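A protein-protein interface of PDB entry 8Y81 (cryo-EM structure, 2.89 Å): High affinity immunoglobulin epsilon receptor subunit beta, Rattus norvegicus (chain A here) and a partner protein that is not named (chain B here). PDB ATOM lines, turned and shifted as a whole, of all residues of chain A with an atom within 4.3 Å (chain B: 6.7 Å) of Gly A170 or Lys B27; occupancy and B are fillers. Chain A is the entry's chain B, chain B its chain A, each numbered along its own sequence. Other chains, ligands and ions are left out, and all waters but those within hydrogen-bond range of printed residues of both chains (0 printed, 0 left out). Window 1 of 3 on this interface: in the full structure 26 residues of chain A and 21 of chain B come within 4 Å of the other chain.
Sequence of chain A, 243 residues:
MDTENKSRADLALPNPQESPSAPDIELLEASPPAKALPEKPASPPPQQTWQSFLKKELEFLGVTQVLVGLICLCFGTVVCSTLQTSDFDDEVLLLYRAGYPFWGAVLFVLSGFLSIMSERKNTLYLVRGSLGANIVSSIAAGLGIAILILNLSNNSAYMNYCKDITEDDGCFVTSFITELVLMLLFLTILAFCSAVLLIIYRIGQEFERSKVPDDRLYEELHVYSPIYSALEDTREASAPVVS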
ATOM      1  N   TYR A 158     -31.448 -11.645   1.920  1.00  0.00           N
ATOM      2  CA  TYR A 158     -30.421 -12.032   0.959  1.00  0.00           C
ATOM      3  C   TYR A 158     -30.681 -11.412  -0.408  1.00  0.00           C
ATOM      4  O   TYR A 158     -29.769 -10.859  -1.031  1.00  0.00           O
ATOM      5  CB  TYR A 158     -30.349 -13.552   0.842  1.00  0.00           C
ATOM      6  CG  TYR A 158     -29.092 -14.059   0.167  1.00  0.00           C
ATOM      7  CD1 TYR A 158     -27.955 -14.329   0.905  1.00  0.00           C
ATOM      8  CD2 TYR A 158     -29.044 -14.266  -1.206  1.00  0.00           C
ATOM      9  CE1 TYR A 158     -26.812 -14.792   0.307  1.00  0.00           C
ATOM     10  CE2 TYR A 158     -27.902 -14.726  -1.815  1.00  0.00           C
ATOM     11  CZ  TYR A 158     -26.790 -14.987  -1.051  1.00  0.00           C
ATOM     12  OH  TYR A 158     -25.642 -15.450  -1.642  1.00  0.00           O
ATOM     13  N   ASP A 168     -25.740 -15.527  -9.749  1.00  0.00           N
ATOM     14  CA  ASP A 168     -24.780 -16.570  -9.436  1.00  0.00           C
ATOM     15  C   ASP A 168     -25.540 -17.725  -8.798  1.00  0.00           C
ATOM     16  O   ASP A 168     -26.774 -17.768  -8.843  1.00  0.00           O
ATOM     17  CB  ASP A 168     -23.671 -16.021  -8.526  1.00  0.00           C
ATOM     18  CG  ASP A 168     -24.220 -15.251  -7.350  1.00  0.00           C
ATOM     19  OD1 ASP A 168     -25.401 -14.852  -7.404  1.00  0.00           O
ATOM     20  OD2 ASP A 168     -23.475 -15.044  -6.375  1.00  0.00           O
ATOM     21  N   ASP A 169     -24.799 -18.661  -8.206  1.00  0.00           N
ATOM     22  CA  ASP A 169     -25.420 -19.768  -7.493  1.00  0.00           C
ATOM     23  C   ASP A 169     -26.101 -19.303  -6.217  1.00  0.00           C
ATOM     24  O   ASP A 169     -27.078 -19.917  -5.786  1.00  0.00           O
ATOM     25  CB  ASP A 169     -24.372 -20.826  -7.167  1.00  0.00           C
ATOM     26  CG  ASP A 169     -23.529 -21.195  -8.364  1.00  0.00           C
ATOM     27  OD1 ASP A 169     -22.640 -20.405  -8.740  1.00  0.00           O
ATOM     28  OD2 ASP A 169     -23.736 -22.290  -8.914  1.00  0.00           O
ATOM     29  N   GLY A 170     -25.605 -18.227  -5.605  1.00  0.00           N
ATOM     30  CA  GLY A 170     -26.155 -17.785  -4.333  1.00  0.00           C
ATOM     31  C   GLY A 170     -27.563 -17.236  -4.454  1.00  0.00           C
ATOM     32  O   GLY A 170     -28.474 -17.685  -3.756  1.00  0.00           O
ATOM     33  N   CYS A 171     -27.765 -16.276  -5.364  1.00  0.00           N
ATOM     34  CA  CYS A 171     -29.087 -15.681  -5.542  1.00  0.00           C
ATOM     35  C   CYS A 171     -30.067 -16.683  -6.141  1.00  0.00           C
ATOM     36  O   CYS A 171     -31.252 -16.681  -5.795  1.00  0.00           O
ATOM     37  CB  CYS A 171     -28.998 -14.435  -6.423  1.00  0.00           C
ATOM     38  SG  CYS A 171     -27.858 -13.140  -5.861  1.00  0.00           S
ATOM     39  N   PHE A 172     -29.581 -17.571  -7.009  1.00  0.00           N
ATOM     40  CA  PHE A 172     -30.450 -18.571  -7.620  1.00  0.00           C
ATOM     41  C   PHE A 172     -30.900 -19.627  -6.620  1.00  0.00           C
ATOM     42  O   PHE A 172     -32.085 -19.976  -6.576  1.00  0.00           O
ATOM     43  CB  PHE A 172     -29.742 -19.237  -8.788  1.00  0.00           C
ATOM     44  CG  PHE A 172     -30.598 -20.208  -9.518  1.00  0.00           C
ATOM     45  CD1 PHE A 172     -31.668 -19.769 -10.279  1.00  0.00           C
ATOM     46  CD2 PHE A 172     -30.342 -21.562  -9.436  1.00  0.00           C
ATOM     47  CE1 PHE A 172     -32.456 -20.666 -10.950  1.00  0.00           C
ATOM     48  CE2 PHE A 172     -31.131 -22.458 -10.102  1.00  0.00           C
ATOM     49  CZ  PHE A 172     -32.182 -22.011 -10.863  1.00  0.00           C
ATOM     50  N   VAL A 173     -29.968 -20.159  -5.824  1.00  0.00           N
ATOM     51  CA  VAL A 173     -30.327 -21.129  -4.796  1.00  0.00           C
ATOM     52  C   VAL A 173     -31.167 -20.472  -3.706  1.00  0.00           C
ATOM     53  O   VAL A 173     -32.095 -21.094  -3.180  1.00  0.00           O
ATOM     54  CB  VAL A 173     -29.049 -21.813  -4.268  1.00  0.00           C
ATOM     55  CG1 VAL A 173     -29.284 -22.570  -2.980  1.00  0.00           C
ATOM     56  CG2 VAL A 173     -28.548 -22.794  -5.304  1.00  0.00           C
ATOM     57  N   THR A 174     -30.928 -19.192  -3.406  1.00  0.00           N
ATOM     58  CA  THR A 174     -31.773 -18.492  -2.445  1.00  0.00           C
ATOM     59  C   THR A 174     -33.187 -18.279  -2.976  1.00  0.00           C
ATOM     60  O   THR A 174     -34.151 -18.409  -2.223  1.00  0.00           O
ATOM     61  CB  THR A 174     -31.138 -17.162  -2.066  1.00  0.00           C
ATOM     62  OG1 THR A 174     -29.751 -17.371  -1.787  1.00  0.00           O
ATOM     63  CG2 THR A 174     -31.813 -16.584  -0.839  1.00  0.00           C
ATOM     64  N   THR B  25     -23.410  -6.550   5.153  1.00  0.00           N
ATOM     65  CA  THR B  25     -24.223  -5.875   4.153  1.00  0.00           C
ATOM     66  C   THR B  25     -24.448  -6.848   2.993  1.00  0.00           C
ATOM     67  O   THR B  25     -25.241  -7.776   3.115  1.00  0.00           O
ATOM     68  CB  THR B  25     -23.560  -4.564   3.666  1.00  0.00           C
ATOM     69  OG1 THR B  25     -23.052  -3.846   4.795  1.00  0.00           O
ATOM     70  CG2 THR B  25     -24.582  -3.663   2.974  1.00  0.00           C
ATOM     71  N   GLN B  26     -23.718  -6.677   1.894  1.00  0.00           N
ATOM     72  CA  GLN B  26     -23.952  -7.455   0.685  1.00  0.00           C
ATOM     73  C   GLN B  26     -23.286  -8.825   0.806  1.00  0.00           C
ATOM     74  O   GLN B  26     -22.852  -9.243   1.882  1.00  0.00           O
ATOM     75  CB  GLN B  26     -23.465  -6.683  -0.540  1.00  0.00           C
ATOM     76  CG  GLN B  26     -21.959  -6.448  -0.576  1.00  0.00           C
ATOM     77  CD  GLN B  26     -21.517  -5.630  -1.775  1.00  0.00           C
ATOM     78  OE1 GLN B  26     -22.327  -5.267  -2.628  1.00  0.00           O
ATOM     79  NE2 GLN B  26     -20.221  -5.345  -1.850  1.00  0.00           N
ATOM     80  N   LYS B  27     -23.224  -9.555  -0.305  1.00  0.00           N
ATOM     81  CA  LYS B  27     -22.447 -10.782  -0.355  1.00  0.00           C
ATOM     82  C   LYS B  27     -20.963 -10.476  -0.226  1.00  0.00           C
ATOM     83  O   LYS B  27     -20.492  -9.399  -0.598  1.00  0.00           O
ATOM     84  CB  LYS B  27     -22.686 -11.527  -1.663  1.00  0.00           C
ATOM     85  CG  LYS B  27     -24.132 -11.822  -1.989  1.00  0.00           C
ATOM     86  CD  LYS B  27     -24.231 -12.563  -3.314  1.00  0.00           C
ATOM     87  CE  LYS B  27     -23.356 -13.810  -3.319  1.00  0.00           C
ATOM     88  NZ  LYS B  27     -24.018 -14.955  -3.996  1.00  0.00           N
ATOM     89  N   SER B  28     -20.223 -11.436   0.307  1.00  0.00           N
ATOM     90  CA  SER B  28     -18.780 -11.311   0.342  1.00  0.00           C
ATOM     91  C   SER B  28     -18.204 -11.540  -1.048  1.00  0.00           C
ATOM     92  O   SER B  28     -18.818 -12.184  -1.901  1.00  0.00           O
ATOM     93  CB  SER B  28     -18.183 -12.291   1.339  1.00  0.00           C
ATOM     94  OG  SER B  28     -18.539 -11.948   2.662  1.00  0.00           O
ATOM     95  N   VAL B  29     -17.035 -10.955  -1.293  1.00  0.00           N
ATOM     96  CA  VAL B  29     -16.354 -11.059  -2.581  1.00  0.00           C
ATOM     97  C   VAL B  29     -14.941 -11.535  -2.279  1.00  0.00           C
ATOM     98  O   VAL B  29     -14.063 -10.727  -1.969  1.00  0.00           O
ATOM     99  CB  VAL B  29     -16.331  -9.736  -3.357  1.00  0.00           C
ATOM    100  CG1 VAL B  29     -15.709  -9.942  -4.730  1.00  0.00           C
ATOM    101  CG2 VAL B  29     -17.723  -9.141  -3.498  1.00  0.00           C
ATOM    102  N   ASN B  50     -13.923  -9.380   1.172  1.00  0.00           N
ATOM    103  CA  ASN B  50     -14.570  -8.170   0.626  1.00  0.00           C
ATOM    104  C   ASN B  50     -13.682  -7.050   0.083  1.00  0.00           C
ATOM    105  O   ASN B  50     -14.022  -6.420  -0.924  1.00  0.00           O
ATOM    106  CB  ASN B  50     -15.473  -7.541   1.682  1.00  0.00           C
ATOM    107  CG  ASN B  50     -16.728  -8.319   1.899  1.00  0.00           C
ATOM    108  OD1 ASN B  50     -17.580  -8.369   1.020  1.00  0.00           O
ATOM    109  ND2 ASN B  50     -16.857  -8.937   3.059  1.00  0.00           N
ATOM    110  N   PHE B  96     -21.500 -10.118   6.950  1.00  0.00           N
ATOM    111  CA  PHE B  96     -21.669 -10.246   5.513  1.00  0.00           C
ATOM    112  C   PHE B  96     -22.131 -11.658   5.179  1.00  0.00           C
ATOM    113  O   PHE B  96     -22.170 -12.545   6.034  1.00  0.00           O
ATOM    114  CB  PHE B  96     -20.370  -9.924   4.767  1.00  0.00           C
ATOM    115  CG  PHE B  96     -20.239  -8.484   4.376  1.00  0.00           C
ATOM    116  CD1 PHE B  96     -20.044  -8.128   3.054  1.00  0.00           C
ATOM    117  CD2 PHE B  96     -20.270  -7.486   5.336  1.00  0.00           C
ATOM    118  CE1 PHE B  96     -19.912  -6.803   2.687  1.00  0.00           C
ATOM    119  CE2 PHE B  96     -20.137  -6.158   4.980  1.00  0.00           C
ATOM    120  CZ  PHE B  96     -19.958  -5.817   3.653  1.00  0.00           C
ATOM    121  N   TYR B  97     -22.483 -11.858   3.914  1.00  0.00           N
ATOM    122  CA  TYR B  97     -23.011 -13.129   3.452  1.00  0.00           C
ATOM    123  C   TYR B  97     -21.856 -14.012   2.980  1.00  0.00           C
ATOM    124  O   TYR B  97     -20.699 -13.593   2.957  1.00  0.00           O
ATOM    125  CB  TYR B  97     -24.030 -12.891   2.340  1.00  0.00           C
ATOM    126  CG  TYR B  97     -25.430 -12.670   2.856  1.00  0.00           C
ATOM    127  CD1 TYR B  97     -26.146 -11.535   2.499  1.00  0.00           C
ATOM    128  CD2 TYR B  97     -26.020 -13.568   3.730  1.00  0.00           C
ATOM    129  CE1 TYR B  97     -27.418 -11.318   2.980  1.00  0.00           C
ATOM    130  CE2 TYR B  97     -27.293 -13.359   4.212  1.00  0.00           C
ATOM    131  CZ  TYR B  97     -27.987 -12.234   3.836  1.00  0.00           C
ATOM    132  OH  TYR B  97     -29.256 -12.030   4.321  1.00  0.00           O
ATOM    133  N   LYS B  98     -22.159 -15.254   2.617  1.00  0.00           N
ATOM    134  CA  LYS B  98     -21.133 -16.106   2.035  1.00  0.00           C
ATOM    135  C   LYS B  98     -20.819 -15.658   0.616  1.00  0.00           C
ATOM    136  O   LYS B  98     -21.669 -15.113  -0.091  1.00  0.00           O
ATOM    137  CB  LYS B  98     -21.564 -17.570   2.040  1.00  0.00           C
ATOM    138  CG  LYS B  98     -21.361 -18.254   3.372  1.00  0.00           C
ATOM    139  CD  LYS B  98     -21.313 -19.758   3.226  1.00  0.00           C
ATOM    140  CE  LYS B  98     -21.302 -20.428   4.581  1.00  0.00           C
ATOM    141  NZ  LYS B  98     -21.241 -21.902   4.459  1.00  0.00           N
ATOM    142  N   SER B  99     -19.582 -15.884   0.203  1.00  0.00           N
ATOM    143  CA  SER B  99     -19.110 -15.361  -1.064  1.00  0.00           C
ATOM    144  C   SER B  99     -19.418 -16.316  -2.206  1.00  0.00           C
ATOM    145  O   SER B  99     -19.689 -17.500  -2.007  1.00  0.00           O
ATOM    146  CB  SER B  99     -17.607 -15.104  -1.017  1.00  0.00           C
ATOM    147  OG  SER B  99     -16.894 -16.276  -1.349  1.00  0.00           O
ATOM    148  N   LYS B 100     -19.382 -15.772  -3.414  1.00  0.00           N
ATOM    149  CA  LYS B 100     -19.282 -16.605  -4.597  1.00  0.00           C
ATOM    150  C   LYS B 100     -17.931 -17.312  -4.567  1.00  0.00           C
ATOM    151  O   LYS B 100     -16.899 -16.650  -4.398  1.00  0.00           O
ATOM    152  CB  LYS B 100     -19.416 -15.760  -5.860  1.00  0.00           C
ATOM    153  CG  LYS B 100     -19.340 -16.544  -7.152  1.00  0.00           C
ATOM    154  CD  LYS B 100     -18.665 -15.738  -8.247  1.00  0.00           C
ATOM    155  CE  LYS B 100     -19.460 -14.496  -8.593  1.00  0.00           C
ATOM    156  NZ  LYS B 100     -20.613 -14.811  -9.473  1.00  0.00           N
ATOM    157  N   ILE B 198     -24.949 -20.837 -13.895  1.00  0.00           N
ATOM    158  CA  ILE B 198     -25.239 -20.766 -12.470  1.00  0.00           C
ATOM    159  C   ILE B 198     -25.602 -22.134 -11.926  1.00  0.00           C
ATOM    160  O   ILE B 198     -25.948 -22.260 -10.752  1.00  0.00           O
ATOM    161  CB  ILE B 198     -26.347 -19.735 -12.172  1.00  0.00           C
ATOM    162  CG1 ILE B 198     -27.620 -20.028 -12.955  1.00  0.00           C
ATOM    163  CG2 ILE B 198     -25.887 -18.332 -12.511  1.00  0.00           C
ATOM    164  CD1 ILE B 198     -28.793 -19.314 -12.418  1.00  0.00           C
ATOM    165  N   TYR B 200     -26.858 -24.771 -11.009  1.00  0.00           N
ATOM    166  CA  TYR B 200     -27.838 -25.420 -10.147  1.00  0.00           C
ATOM    167  C   TYR B 200     -29.244 -25.382 -10.738  1.00  0.00           C
ATOM    168  O   TYR B 200     -30.210 -25.508  -9.980  1.00  0.00           O
ATOM    169  CB  TYR B 200     -27.866 -24.765  -8.759  1.00  0.00           C
ATOM    170  CG  TYR B 200     -26.911 -25.381  -7.765  1.00  0.00           C
ATOM    171  CD1 TYR B 200     -27.122 -26.660  -7.274  1.00  0.00           C
ATOM    172  CD2 TYR B 200     -25.805 -24.678  -7.312  1.00  0.00           C
ATOM    173  CE1 TYR B 200     -26.252 -27.226  -6.365  1.00  0.00           C
ATOM    174  CE2 TYR B 200     -24.930 -25.236  -6.405  1.00  0.00           C
ATOM    175  CZ  TYR B 200     -25.160 -26.508  -5.932  1.00  0.00           C
ATOM    176  OH  TYR B 200     -24.290 -27.067  -5.026  1.00  0.00           O
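OD2 of Asp A169 lies close to O of Ile B198. NZ of Lys B27 sits at hydrogen-bond distance from OH of Tyr A158 (2.9 Å). The side-chain hydroxyl (OH) of Tyr B97 is in hydrogen-bond range of the backbone NH (N) of Tyr A158 (3.3 Å). OD2 of Asp A168 lies within salt-bridge range of NZ of Lys B27, 2.4 Å away.
The backbone carbonyl oxygen (O) of Lys B27 sits close to the side-chain amide oxygen (OD1) of Asn B50 (3.5 Å). The backbone NH (N) of Tyr B97 lies within hydrogen-bond range of the backbone carbonyl oxygen (O) of Gln B26 (3.3 Å). The backbone NH of Cys A171 lies within hydrogen-bond range of the side-chain carboxylate of Asp A168. The backbone carbonyl oxygen of Tyr B97 lies within hydrogen-bond range of the side-chain hydroxyl of Ser B28 (2.7 Å).
NZ of Lys B100 touches CB of Asp A168 (3.4 Å). CG2 of Ile B198 touches CA of Asp A168, at 3.7 Å. Tyr B200 touches Asp A169 (CD2 to OD2, 3.5 Å). NZ of Lys B27 touches CA of Gly A170 (3.6 Å). Phe A172 touches Ile B198 (CG to CD1, 3.5 Å). CE2 of Phe A172 touches O of Tyr B200, 3.2 Å away. Tyr B200 touches Val A173.
Printed residues of chain B within 4 Å of Gly A170: Lys B27. Of chain A, only Tyr A158 (2.9 Å), Asp A168 (2.4 Å) and Gly A170 (3.6 Å) come within 4 Å of Lys B27. Of the printed residues of chain B, Phe A172 touches Ile B198 and Tyr B200. Printed residues of chain B within 4 Å of Asp A169: Ile B198 (2.9 Å) and Tyr B200 (3.5 Å). Of the printed residues of chain A, Tyr B200 touches Asp A169, Phe A172 and Val A173. Printed residues of chain A within 4 Å of Tyr B97: Tyr A158 (3.3 Å). Of the printed residues of chain A, Ile B198 touches Asp A168, Asp A169 and Phe A172. Thr A174 touches none of the printed residues of chain B. The nearest residue of chain A that does not touch Lys B27 is Cys A171 (4.2 Å).
Printed residues of chain A that touch a printed residue of chain B: Tyr A158, Asp A168, Asp A169, Gly A170, Phe A172 and Val A173. Along chain A the printed residues that touch a printed residue of chain B span positions 158 to 173. Among the printed residues, Asp or Glu carboxylates within 4 Å of a Lys or Arg side-chain nitrogen of the other chain: Asp A168 with Lys B27 (2.4 Å).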
